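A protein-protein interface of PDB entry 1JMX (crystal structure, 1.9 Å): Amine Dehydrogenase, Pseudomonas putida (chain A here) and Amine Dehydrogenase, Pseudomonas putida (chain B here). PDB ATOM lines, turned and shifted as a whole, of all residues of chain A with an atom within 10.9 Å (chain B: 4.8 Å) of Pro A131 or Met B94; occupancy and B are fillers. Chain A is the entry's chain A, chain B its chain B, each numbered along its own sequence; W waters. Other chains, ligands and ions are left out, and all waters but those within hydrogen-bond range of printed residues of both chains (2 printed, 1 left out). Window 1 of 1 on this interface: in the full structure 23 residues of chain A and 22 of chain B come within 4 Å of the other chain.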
ATOM      1  N   MET A  47      -1.458 -15.064 -35.627  1.00  0.00           N
ATOM      2  CA  MET A  47      -1.681 -16.483 -35.383  1.00  0.00           C
ATOM      3  C   MET A  47      -1.468 -17.413 -36.559  1.00  0.00           C
ATOM      4  O   MET A  47      -0.881 -18.477 -36.402  1.00  0.00           O
ATOM      5  CB  MET A  47      -3.099 -16.708 -34.855  1.00  0.00           C
ATOM      6  CG  MET A  47      -3.394 -16.006 -33.547  1.00  0.00           C
ATOM      7  SD  MET A  47      -5.074 -16.267 -32.947  1.00  0.00           S
ATOM      8  CE  MET A  47      -5.020 -15.222 -31.467  1.00  0.00           C
ATOM      9  N   ARG A 102     -14.833 -12.472 -18.806  1.00  0.00           N
ATOM     10  CA  ARG A 102     -13.873 -12.533 -17.708  1.00  0.00           C
ATOM     11  C   ARG A 102     -12.425 -12.312 -18.146  1.00  0.00           C
ATOM     12  O   ARG A 102     -11.540 -12.132 -17.319  1.00  0.00           O
ATOM     13  CB  ARG A 102     -14.006 -13.851 -16.943  1.00  0.00           C
ATOM     14  CG  ARG A 102     -13.612 -15.072 -17.730  1.00  0.00           C
ATOM     15  CD  ARG A 102     -13.592 -16.290 -16.842  1.00  0.00           C
ATOM     16  NE  ARG A 102     -13.262 -17.503 -17.582  1.00  0.00           N
ATOM     17  CZ  ARG A 102     -12.029 -17.883 -17.916  1.00  0.00           C
ATOM     18  NH1 ARG A 102     -10.977 -17.147 -17.586  1.00  0.00           N
ATOM     19  NH2 ARG A 102     -11.848 -19.039 -18.547  1.00  0.00           N
ATOM     20  N   CYS A 103     -12.206 -12.298 -19.452  1.00  0.00           N
ATOM     21  CA  CYS A 103     -10.884 -12.093 -20.029  1.00  0.00           C
ATOM     22  C   CYS A 103     -10.881 -10.708 -20.652  1.00  0.00           C
ATOM     23  O   CYS A 103     -10.164  -9.812 -20.208  1.00  0.00           O
ATOM     24  CB  CYS A 103     -10.646 -13.152 -21.098  1.00  0.00           C
ATOM     25  SG  CYS A 103     -10.031 -14.687 -20.434  1.00  0.00           S
ATOM     26  N   VAL A 123     -16.213 -20.747 -30.044  1.00  0.00           N
ATOM     27  CA  VAL A 123     -15.931 -21.436 -28.783  1.00  0.00           C
ATOM     28  C   VAL A 123     -14.777 -22.441 -28.934  1.00  0.00           C
ATOM     29  O   VAL A 123     -13.885 -22.498 -28.088  1.00  0.00           O
ATOM     30  CB  VAL A 123     -17.176 -22.159 -28.233  1.00  0.00           C
ATOM     31  CG1 VAL A 123     -16.816 -22.962 -26.997  1.00  0.00           C
ATOM     32  CG2 VAL A 123     -18.249 -21.151 -27.888  1.00  0.00           C
ATOM     33  N   ASN A 124     -14.787 -23.212 -30.022  1.00  0.00           N
ATOM     34  CA  ASN A 124     -13.734 -24.193 -30.287  1.00  0.00           C
ATOM     35  C   ASN A 124     -12.383 -23.522 -30.471  1.00  0.00           C
ATOM     36  O   ASN A 124     -11.368 -24.051 -30.035  1.00  0.00           O
ATOM     37  CB  ASN A 124     -14.075 -25.042 -31.517  1.00  0.00           C
ATOM     38  CG  ASN A 124     -15.072 -26.133 -31.206  1.00  0.00           C
ATOM     39  OD1 ASN A 124     -14.717 -27.169 -30.661  1.00  0.00           O
ATOM     40  ND2 ASN A 124     -16.328 -25.896 -31.535  1.00  0.00           N
ATOM     41  N   PHE A 125     -12.375 -22.359 -31.119  1.00  0.00           N
ATOM     42  CA  PHE A 125     -11.141 -21.612 -31.325  1.00  0.00           C
ATOM     43  C   PHE A 125     -10.533 -21.168 -29.997  1.00  0.00           C
ATOM     44  O   PHE A 125      -9.325 -21.207 -29.830  1.00  0.00           O
ATOM     45  CB  PHE A 125     -11.368 -20.379 -32.207  1.00  0.00           C
ATOM     46  CG  PHE A 125     -10.287 -19.328 -32.072  1.00  0.00           C
ATOM     47  CD1 PHE A 125     -10.516 -18.164 -31.338  1.00  0.00           C
ATOM     48  CD2 PHE A 125      -9.025 -19.529 -32.626  1.00  0.00           C
ATOM     49  CE1 PHE A 125      -9.509 -17.231 -31.157  1.00  0.00           C
ATOM     50  CE2 PHE A 125      -8.010 -18.596 -32.446  1.00  0.00           C
ATOM     51  CZ  PHE A 125      -8.254 -17.448 -31.710  1.00  0.00           C
ATOM     52  N   HIS A 126     -11.371 -20.707 -29.074  1.00  0.00           N
ATOM     53  CA  HIS A 126     -10.892 -20.254 -27.775  1.00  0.00           C
ATOM     54  C   HIS A 126     -10.192 -21.352 -26.998  1.00  0.00           C
ATOM     55  O   HIS A 126      -9.031 -21.201 -26.620  1.00  0.00           O
ATOM     56  CB  HIS A 126     -12.041 -19.675 -26.949  1.00  0.00           C
ATOM     57  CG  HIS A 126     -12.395 -18.274 -27.324  1.00  0.00           C
ATOM     58  ND1 HIS A 126     -13.175 -17.934 -28.407  1.00  0.00           N
ATOM     59  CD2 HIS A 126     -12.012 -17.102 -26.767  1.00  0.00           C
ATOM     60  CE1 HIS A 126     -13.229 -16.614 -28.476  1.00  0.00           C
ATOM     61  NE2 HIS A 126     -12.540 -16.070 -27.500  1.00  0.00           N
ATOM     62  N   LEU A 127     -10.898 -22.456 -26.767  1.00  0.00           N
ATOM     63  CA  LEU A 127     -10.335 -23.582 -26.030  1.00  0.00           C
ATOM     64  C   LEU A 127      -9.176 -24.219 -26.807  1.00  0.00           C
ATOM     65  O   LEU A 127      -8.281 -24.802 -26.212  1.00  0.00           O
ATOM     66  CB  LEU A 127     -11.414 -24.634 -25.742  1.00  0.00           C
ATOM     67  CG  LEU A 127     -11.420 -25.337 -24.379  1.00  0.00           C
ATOM     68  CD1 LEU A 127     -12.239 -26.596 -24.489  1.00  0.00           C
ATOM     69  CD2 LEU A 127     -10.027 -25.670 -23.888  1.00  0.00           C
ATOM     70  N   GLY A 128      -9.194 -24.083 -28.132  1.00  0.00           N
ATOM     71  CA  GLY A 128      -8.135 -24.643 -28.953  1.00  0.00           C
ATOM     72  C   GLY A 128      -6.861 -23.824 -28.935  1.00  0.00           C
ATOM     73  O   GLY A 128      -5.770 -24.374 -28.829  1.00  0.00           O
ATOM     74  N   GLN A 129      -7.015 -22.504 -29.029  1.00  0.00           N
ATOM     75  CA  GLN A 129      -5.894 -21.570 -29.025  1.00  0.00           C
ATOM     76  C   GLN A 129      -5.303 -21.383 -27.617  1.00  0.00           C
ATOM     77  O   GLN A 129      -4.096 -21.190 -27.463  1.00  0.00           O
ATOM     78  CB  GLN A 129      -6.343 -20.219 -29.595  1.00  0.00           C
ATOM     79  CG  GLN A 129      -5.203 -19.253 -29.906  1.00  0.00           C
ATOM     80  CD  GLN A 129      -4.307 -19.748 -31.026  1.00  0.00           C
ATOM     81  OE1 GLN A 129      -4.696 -20.611 -31.805  1.00  0.00           O
ATOM     82  NE2 GLN A 129      -3.100 -19.205 -31.107  1.00  0.00           N
ATOM     83  N   TRP A 130      -6.164 -21.435 -26.602  1.00  0.00           N
ATOM     84  CA  TRP A 130      -5.740 -21.288 -25.214  1.00  0.00           C
ATOM     85  C   TRP A 130      -6.262 -22.475 -24.411  1.00  0.00           C
ATOM     86  O   TRP A 130      -7.304 -22.388 -23.771  1.00  0.00           O
ATOM     87  CB  TRP A 130      -6.259 -19.971 -24.626  1.00  0.00           C
ATOM     88  CG  TRP A 130      -5.794 -18.794 -25.392  1.00  0.00           C
ATOM     89  CD1 TRP A 130      -4.521 -18.340 -25.480  1.00  0.00           C
ATOM     90  CD2 TRP A 130      -6.570 -17.996 -26.295  1.00  0.00           C
ATOM     91  NE1 TRP A 130      -4.442 -17.322 -26.394  1.00  0.00           N
ATOM     92  CE2 TRP A 130      -5.686 -17.090 -26.913  1.00  0.00           C
ATOM     93  CE3 TRP A 130      -7.925 -17.970 -26.650  1.00  0.00           C
ATOM     94  CZ2 TRP A 130      -6.105 -16.166 -27.874  1.00  0.00           C
ATOM     95  CZ3 TRP A 130      -8.347 -17.050 -27.606  1.00  0.00           C
ATOM     96  CH2 TRP A 130      -7.435 -16.162 -28.208  1.00  0.00           C
ATOM     97  N   PRO A 131      -5.539 -23.613 -24.450  1.00  0.00           N
ATOM     98  CA  PRO A 131      -5.909 -24.840 -23.734  1.00  0.00           C
ATOM     99  C   PRO A 131      -6.153 -24.668 -22.231  1.00  0.00           C
ATOM    100  O   PRO A 131      -6.951 -25.389 -21.652  1.00  0.00           O
ATOM    101  CB  PRO A 131      -4.717 -25.764 -24.011  1.00  0.00           C
ATOM    102  CG  PRO A 131      -4.256 -25.322 -25.355  1.00  0.00           C
ATOM    103  CD  PRO A 131      -4.296 -23.821 -25.216  1.00  0.00           C
ATOM    104  N   SER A 132      -5.487 -23.701 -21.612  1.00  0.00           N
ATOM    105  CA  SER A 132      -5.643 -23.467 -20.180  1.00  0.00           C
ATOM    106  C   SER A 132      -6.966 -22.802 -19.814  1.00  0.00           C
ATOM    107  O   SER A 132      -7.293 -22.678 -18.638  1.00  0.00           O
ATOM    108  CB  SER A 132      -4.505 -22.596 -19.661  1.00  0.00           C
ATOM    109  OG  SER A 132      -4.610 -21.294 -20.198  1.00  0.00           O
ATOM    110  N   LEU A 133      -7.717 -22.372 -20.822  1.00  0.00           N
ATOM    111  CA  LEU A 133      -8.995 -21.703 -20.621  1.00  0.00           C
ATOM    112  C   LEU A 133      -9.910 -22.392 -19.607  1.00  0.00           C
ATOM    113  O   LEU A 133     -10.368 -21.760 -18.658  1.00  0.00           O
ATOM    114  CB  LEU A 133      -9.712 -21.537 -21.965  1.00  0.00           C
ATOM    115  CG  LEU A 133     -10.938 -20.627 -22.095  1.00  0.00           C
ATOM    116  CD1 LEU A 133     -11.137 -20.263 -23.554  1.00  0.00           C
ATOM    117  CD2 LEU A 133     -12.175 -21.288 -21.536  1.00  0.00           C
ATOM    118  N   GLU A 134     -10.135 -23.691 -19.793  1.00  0.00           N
ATOM    119  CA  GLU A 134     -11.014 -24.471 -18.920  1.00  0.00           C
ATOM    120  C   GLU A 134     -10.462 -24.820 -17.530  1.00  0.00           C
ATOM    121  O   GLU A 134     -11.126 -25.491 -16.742  1.00  0.00           O
ATOM    122  CB  GLU A 134     -11.459 -25.743 -19.648  1.00  0.00           C
ATOM    123  CG  GLU A 134     -10.319 -26.704 -19.954  1.00  0.00           C
ATOM    124  CD  GLU A 134     -10.744 -27.871 -20.820  1.00  0.00           C
ATOM    125  OE1 GLU A 134     -11.898 -28.334 -20.700  1.00  0.00           O
ATOM    126  OE2 GLU A 134      -9.918 -28.320 -21.634  1.00  0.00           O
ATOM    127  N   TYR A 135      -9.250 -24.361 -17.233  1.00  0.00           N
ATOM    128  CA  TYR A 135      -8.626 -24.611 -15.937  1.00  0.00           C
ATOM    129  C   TYR A 135      -8.574 -23.331 -15.119  1.00  0.00           C
ATOM    130  O   TYR A 135      -8.197 -23.353 -13.955  1.00  0.00           O
ATOM    131  CB  TYR A 135      -7.198 -25.139 -16.112  1.00  0.00           C
ATOM    132  CG  TYR A 135      -7.107 -26.487 -16.774  1.00  0.00           C
ATOM    133  CD1 TYR A 135      -7.006 -27.650 -16.014  1.00  0.00           C
ATOM    134  CD2 TYR A 135      -7.113 -26.605 -18.163  1.00  0.00           C
ATOM    135  CE1 TYR A 135      -6.911 -28.895 -16.616  1.00  0.00           C
ATOM    136  CE2 TYR A 135      -7.023 -27.847 -18.775  1.00  0.00           C
ATOM    137  CZ  TYR A 135      -6.922 -28.985 -17.996  1.00  0.00           C
ATOM    138  OH  TYR A 135      -6.833 -30.213 -18.595  1.00  0.00           O
ATOM    139  N   GLN A 136      -8.936 -22.216 -15.750  1.00  0.00           N
ATOM    140  CA  GLN A 136      -8.914 -20.907 -15.110  1.00  0.00           C
ATOM    141  C   GLN A 136     -10.132 -20.671 -14.224  1.00  0.00           C
ATOM    142  O   GLN A 136     -11.084 -21.448 -14.256  1.00  0.00           O
ATOM    143  CB  GLN A 136      -8.814 -19.812 -16.181  1.00  0.00           C
ATOM    144  CG  GLN A 136      -7.522 -19.850 -16.992  1.00  0.00           C
ATOM    145  CD  GLN A 136      -7.562 -18.966 -18.222  1.00  0.00           C
ATOM    146  OE1 GLN A 136      -8.501 -18.210 -18.426  1.00  0.00           O
ATOM    147  NE2 GLN A 136      -6.541 -19.069 -19.054  1.00  0.00           N
ATOM    148  N   ALA A 137     -10.086 -19.604 -13.425  1.00  0.00           N
ATOM    149  CA  ALA A 137     -11.192 -19.249 -12.535  1.00  0.00           C
ATOM    150  C   ALA A 137     -12.466 -19.062 -13.350  1.00  0.00           C
ATOM    151  O   ALA A 137     -12.428 -18.494 -14.447  1.00  0.00           O
ATOM    152  CB  ALA A 137     -10.869 -17.975 -11.767  1.00  0.00           C
ATOM    153  N   ALA A 139     -14.147 -21.438 -14.665  1.00  0.00           N
ATOM    154  CA  ALA A 139     -14.113 -22.426 -15.726  1.00  0.00           C
ATOM    155  C   ALA A 139     -13.836 -23.804 -15.118  1.00  0.00           C
ATOM    156  O   ALA A 139     -14.510 -24.763 -15.453  1.00  0.00           O
ATOM    157  CB  ALA A 139     -13.049 -22.065 -16.744  1.00  0.00           C
ATOM    158  N   ARG A 140     -12.870 -23.877 -14.198  1.00  0.00           N
ATOM    159  CA  ARG A 140     -12.482 -25.125 -13.519  1.00  0.00           C
ATOM    160  C   ARG A 140     -13.557 -25.634 -12.545  1.00  0.00           C
ATOM    161  O   ARG A 140     -13.466 -26.743 -12.023  1.00  0.00           O
ATOM    162  CB  ARG A 140     -11.172 -24.921 -12.735  1.00  0.00           C
ATOM    163  CG  ARG A 140     -11.356 -24.163 -11.413  1.00  0.00           C
ATOM    164  CD  ARG A 140     -10.108 -24.157 -10.533  1.00  0.00           C
ATOM    165  NE  ARG A 140      -9.079 -23.293 -11.086  1.00  0.00           N
ATOM    166  CZ  ARG A 140      -8.668 -22.138 -10.563  1.00  0.00           C
ATOM    167  NH1 ARG A 140      -9.175 -21.674  -9.436  1.00  0.00           N
ATOM    168  NH2 ARG A 140      -7.800 -21.398 -11.238  1.00  0.00           N
ATOM    169  N   TRP A 144     -16.987 -26.539 -18.493  1.00  0.00           N
ATOM    170  CA  TRP A 144     -16.935 -25.395 -19.391  1.00  0.00           C
ATOM    171  C   TRP A 144     -17.357 -25.611 -20.839  1.00  0.00           C
ATOM    172  O   TRP A 144     -18.219 -24.893 -21.338  1.00  0.00           O
ATOM    173  CB  TRP A 144     -15.555 -24.735 -19.340  1.00  0.00           C
ATOM    174  CG  TRP A 144     -15.586 -23.339 -19.861  1.00  0.00           C
ATOM    175  CD1 TRP A 144     -15.860 -22.213 -19.151  1.00  0.00           C
ATOM    176  CD2 TRP A 144     -15.420 -22.927 -21.223  1.00  0.00           C
ATOM    177  NE1 TRP A 144     -15.890 -21.124 -19.982  1.00  0.00           N
ATOM    178  CE2 TRP A 144     -15.623 -21.532 -21.262  1.00  0.00           C
ATOM    179  CE3 TRP A 144     -15.121 -23.600 -22.415  1.00  0.00           C
ATOM    180  CZ2 TRP A 144     -15.541 -20.795 -22.448  1.00  0.00           C
ATOM    181  CZ3 TRP A 144     -15.037 -22.868 -23.593  1.00  0.00           C
ATOM    182  CH2 TRP A 144     -15.246 -21.480 -23.601  1.00  0.00           C
ATOM    183  N   LEU A 145     -16.756 -26.586 -21.513  1.00  0.00           N
ATOM    184  CA  LEU A 145     -17.082 -26.838 -22.917  1.00  0.00           C
ATOM    185  C   LEU A 145     -18.567 -27.171 -23.179  1.00  0.00           C
ATOM    186  O   LEU A 145     -19.202 -26.516 -24.011  1.00  0.00           O
ATOM    187  CB  LEU A 145     -16.126 -27.879 -23.516  1.00  0.00           C
ATOM    188  CG  LEU A 145     -16.132 -28.113 -25.029  1.00  0.00           C
ATOM    189  CD1 LEU A 145     -15.963 -26.793 -25.786  1.00  0.00           C
ATOM    190  CD2 LEU A 145     -15.024 -29.095 -25.370  1.00  0.00           C
ATOM    191  N   TYR B  64       4.361 -27.061 -23.527  1.00  0.00           N
ATOM    192  CA  TYR B  64       3.386 -28.078 -23.120  1.00  0.00           C
ATOM    193  C   TYR B  64       3.040 -29.097 -24.207  1.00  0.00           C
ATOM    194  O   TYR B  64       1.955 -29.673 -24.194  1.00  0.00           O
ATOM    195  CB  TYR B  64       2.094 -27.398 -22.636  1.00  0.00           C
ATOM    196  CG  TYR B  64       2.291 -26.347 -21.557  1.00  0.00           C
ATOM    197  CD1 TYR B  64       2.872 -25.111 -21.850  1.00  0.00           C
ATOM    198  CD2 TYR B  64       1.903 -26.593 -20.240  1.00  0.00           C
ATOM    199  CE1 TYR B  64       3.065 -24.156 -20.866  1.00  0.00           C
ATOM    200  CE2 TYR B  64       2.090 -25.641 -19.246  1.00  0.00           C
ATOM    201  CZ  TYR B  64       2.674 -24.424 -19.564  1.00  0.00           C
ATOM    202  OH  TYR B  64       2.884 -23.491 -18.574  1.00  0.00           O
ATOM    203  N   ARG B  92      -1.692 -30.823 -26.325  1.00  0.00           N
ATOM    204  CA  ARG B  92      -1.103 -30.103 -25.207  1.00  0.00           C
ATOM    205  C   ARG B  92      -1.365 -30.816 -23.886  1.00  0.00           C
ATOM    206  O   ARG B  92      -2.421 -31.395 -23.675  1.00  0.00           O
ATOM    207  CB  ARG B  92      -1.673 -28.690 -25.122  1.00  0.00           C
ATOM    208  CG  ARG B  92      -0.690 -27.610 -25.477  1.00  0.00           C
ATOM    209  CD  ARG B  92      -0.743 -27.261 -26.941  1.00  0.00           C
ATOM    210  NE  ARG B  92       0.605 -27.194 -27.492  1.00  0.00           N
ATOM    211  CZ  ARG B  92       1.066 -26.209 -28.256  1.00  0.00           C
ATOM    212  NH1 ARG B  92       0.296 -25.173 -28.571  1.00  0.00           N
ATOM    213  NH2 ARG B  92       2.301 -26.285 -28.731  1.00  0.00           N
ATOM    214  N   SER B  93      -0.398 -30.752 -22.987  1.00  0.00           N
ATOM    215  CA  SER B  93      -0.543 -31.373 -21.685  1.00  0.00           C
ATOM    216  C   SER B  93      -0.521 -30.300 -20.578  1.00  0.00           C
ATOM    217  O   SER B  93       0.470 -29.595 -20.404  1.00  0.00           O
ATOM    218  CB  SER B  93       0.570 -32.398 -21.481  1.00  0.00           C
ATOM    219  OG  SER B  93       0.518 -32.959 -20.186  1.00  0.00           O
ATOM    220  N   MET B  94      -1.628 -30.168 -19.852  1.00  0.00           N
ATOM    221  CA  MET B  94      -1.723 -29.192 -18.768  1.00  0.00           C
ATOM    222  C   MET B  94      -1.058 -29.746 -17.512  1.00  0.00           C
ATOM    223  O   MET B  94      -1.741 -30.096 -16.547  1.00  0.00           O
ATOM    224  CB  MET B  94      -3.191 -28.851 -18.479  1.00  0.00           C
ATOM    225  CG  MET B  94      -3.401 -27.575 -17.673  1.00  0.00           C
ATOM    226  SD  MET B  94      -2.764 -26.100 -18.509  1.00  0.00           S
ATOM    227  CE  MET B  94      -3.291 -26.405 -20.178  1.00  0.00           C
ATOM    228  N   TYR B  95       0.276 -29.816 -17.539  1.00  0.00           N
ATOM    229  CA  TYR B  95       1.075 -30.343 -16.428  1.00  0.00           C
ATOM    230  C   TYR B  95       0.699 -31.799 -16.104  1.00  0.00           C
ATOM    231  O   TYR B  95       0.963 -32.272 -15.001  1.00  0.00           O
ATOM    232  CB  TYR B  95       0.896 -29.474 -15.174  1.00  0.00           C
ATOM    233  CG  TYR B  95       1.371 -28.051 -15.332  1.00  0.00           C
ATOM    234  CD1 TYR B  95       0.503 -27.046 -15.757  1.00  0.00           C
ATOM    235  CD2 TYR B  95       2.689 -27.712 -15.075  1.00  0.00           C
ATOM    236  CE1 TYR B  95       0.940 -25.739 -15.926  1.00  0.00           C
ATOM    237  CE2 TYR B  95       3.140 -26.407 -15.239  1.00  0.00           C
ATOM    238  CZ  TYR B  95       2.263 -25.425 -15.668  1.00  0.00           C
ATOM    239  OH  TYR B  95       2.724 -24.143 -15.865  1.00  0.00           O
ATOM    240  N   SER B  96       0.133 -32.507 -17.085  1.00  0.00           N
ATOM    241  CA  SER B  96      -0.326 -33.879 -16.891  1.00  0.00           C
ATOM    242  C   SER B  96       0.568 -34.976 -17.450  1.00  0.00           C
ATOM    243  O   SER B  96       0.384 -35.415 -18.582  1.00  0.00           O
ATOM    244  CB  SER B  96      -1.748 -34.042 -17.441  1.00  0.00           C
ATOM    245  N   ASN B 111      -4.775 -33.022 -24.366  1.00  0.00           N
ATOM    246  CA  ASN B 111      -5.968 -32.255 -24.720  1.00  0.00           C
ATOM    247  C   ASN B 111      -5.641 -31.836 -26.158  1.00  0.00           C
ATOM    248  O   ASN B 111      -4.888 -30.890 -26.375  1.00  0.00           O
ATOM    249  CB  ASN B 111      -6.102 -30.996 -23.840  1.00  0.00           C
ATOM    250  CG  ASN B 111      -6.320 -31.308 -22.359  1.00  0.00           C
ATOM    251  OD1 ASN B 111      -6.225 -30.419 -21.515  1.00  0.00           O
ATOM    252  ND2 ASN B 111      -6.640 -32.551 -22.046  1.00  0.00           N
ATOM    253  N   VAL B 150      -8.265 -32.342 -16.706  1.00  0.00           N
ATOM    254  CA  VAL B 150      -7.306 -33.167 -15.988  1.00  0.00           C
ATOM    255  C   VAL B 150      -5.953 -32.459 -16.006  1.00  0.00           C
ATOM    256  O   VAL B 150      -5.554 -31.900 -17.021  1.00  0.00           O
ATOM    257  CB  VAL B 150      -7.189 -34.589 -16.621  1.00  0.00           C
ATOM    258  CG1 VAL B 150      -5.902 -35.278 -16.191  1.00  0.00           C
ATOM    259  CG2 VAL B 150      -8.400 -35.441 -16.238  1.00  0.00           C
ATOM    260  N   TYR B 151      -5.290 -32.422 -14.852  1.00  0.00           N
ATOM    261  CA  TYR B 151      -3.976 -31.809 -14.734  1.00  0.00           C
ATOM    262  C   TYR B 151      -2.982 -32.781 -14.079  1.00  0.00           C
ATOM    263  O   TYR B 151      -2.720 -33.831 -14.650  1.00  0.00           O
ATOM    264  CB  TYR B 151      -4.052 -30.428 -14.051  1.00  0.00           C
ATOM    265  CG  TYR B 151      -4.781 -30.365 -12.719  1.00  0.00           C
ATOM    266  CD1 TYR B 151      -4.075 -30.176 -11.528  1.00  0.00           C
ATOM    267  CD2 TYR B 151      -6.171 -30.488 -12.644  1.00  0.00           C
ATOM    268  CE1 TYR B 151      -4.726 -30.118 -10.303  1.00  0.00           C
ATOM    269  CE2 TYR B 151      -6.831 -30.430 -11.418  1.00  0.00           C
ATOM    270  CZ  TYR B 151      -6.097 -30.249 -10.251  1.00  0.00           C
ATOM    271  OH  TYR B 151      -6.720 -30.240  -9.021  1.00  0.00           O
ATOM    272  N   LEU B 152      -2.463 -32.478 -12.892  1.00  0.00           N
ATOM    273  CA  LEU B 152      -1.499 -33.349 -12.209  1.00  0.00           C
ATOM    274  C   LEU B 152      -1.852 -34.840 -12.068  1.00  0.00           C
ATOM    275  O   LEU B 152      -2.992 -35.207 -11.795  1.00  0.00           O
ATOM    276  CB  LEU B 152      -1.162 -32.792 -10.828  1.00  0.00           C
ATOM    277  CG  LEU B 152      -0.532 -31.406 -10.799  1.00  0.00           C
ATOM    278  CD1 LEU B 152      -0.176 -31.060  -9.372  1.00  0.00           C
ATOM    279  CD2 LEU B 152       0.691 -31.376 -11.675  1.00  0.00           C
ATOM    280  N   PHE B 200      -0.010 -26.728 -10.051  1.00  0.00           N
ATOM    281  CA  PHE B 200       0.824 -27.129 -11.179  1.00  0.00           C
ATOM    282  C   PHE B 200       2.185 -27.606 -10.699  1.00  0.00           C
ATOM    283  O   PHE B 200       3.143 -27.639 -11.466  1.00  0.00           O
ATOM    284  CB  PHE B 200       1.030 -25.945 -12.121  1.00  0.00           C
ATOM    285  CG  PHE B 200      -0.245 -25.349 -12.625  1.00  0.00           C
ATOM    286  CD1 PHE B 200      -1.287 -26.171 -13.058  1.00  0.00           C
ATOM    287  CD2 PHE B 200      -0.420 -23.971 -12.642  1.00  0.00           C
ATOM    288  CE1 PHE B 200      -2.485 -25.626 -13.494  1.00  0.00           C
ATOM    289  CE2 PHE B 200      -1.611 -23.416 -13.076  1.00  0.00           C
ATOM    290  CZ  PHE B 200      -2.646 -24.240 -13.501  1.00  0.00           C
HETATM  291  O   HOH W   1      -7.895 -33.392 -19.600  1.00  0.00           O
HETATM  292  O   HOH W   2      -9.481 -30.952 -20.921  1.00  0.00           O
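NE2 of Gln A136 lies within hydrogen-bond range of OG of Ser A132 (3.2 Å). The backbone NH (N) of Asn B111 is in hydrogen-bond range of the backbone carbonyl oxygen (O) of Arg B92, at 2.9 Å. NE of Arg A140 lies within hydrogen-bond range of O of Tyr A135 (3.0 Å).
Among the printed residues, merely in contact across the chains: Pro A131 with Met B94 (3.9 Å), Ser A132 with Met B94 (3.8 Å) and Tyr A135 with Met B94 (3.8 Å).
The side-chain hydroxyl (OH) of Tyr A135 sits at hydrogen-bond distance from the backbone carbonyl oxygen (O) of Val B150 (2.6 Å). OH of Tyr A135 lies within hydrogen-bond range of OD1 of Asn B111 (3.0 Å).
Water W2 bridges the side-chain carboxylate (OE2) of Glu A134 (2.8 Å) and the side-chain amide oxygen (OD1) of Asn B111 (3.4 Å). Water W1 lies within hydrogen-bond range of ND2 of Asn B111 (2.9 Å), N of Val B150 (3.1 Å) and OH of Tyr A135 (3.5 Å).
Hydrophobic or aromatic side chains of chain B within 4 Å of the printed part of chain A: Met B94. Among the printed residues, 5 pairs touch across the chains. Among the printed residues, no Asp or Glu carboxylate lies within 4 Å of a Lys or Arg side-chain nitrogen of the other chain.
Pro A131 touches just one residue of chain B: Met B94. Printed residues of chain B within 4 Å of Ser A132: Met B94 (3.8 Å). Of the printed residues of chain B, Tyr A135 touches Met B94, Asn B111 and Val B150. Ala A137 touches none of the printed residues of chain B. No residue of chain A comes within 4 Å of Ser B93. Of chain A, only Pro A131 (3.9 Å), Ser A132 (3.8 Å) and Tyr A135 (3.8 Å) come within 4 Å of Met B94. No residue of chain A comes within 4 Å of Tyr B95. Of chain A, only Tyr A135 comes within 4 Å of Asn B111. Of the printed residues of chain A, Val B150 touches Tyr A135. The nearest residue of chain A that does not touch Met B94 is Leu A133 (6.0 Å).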
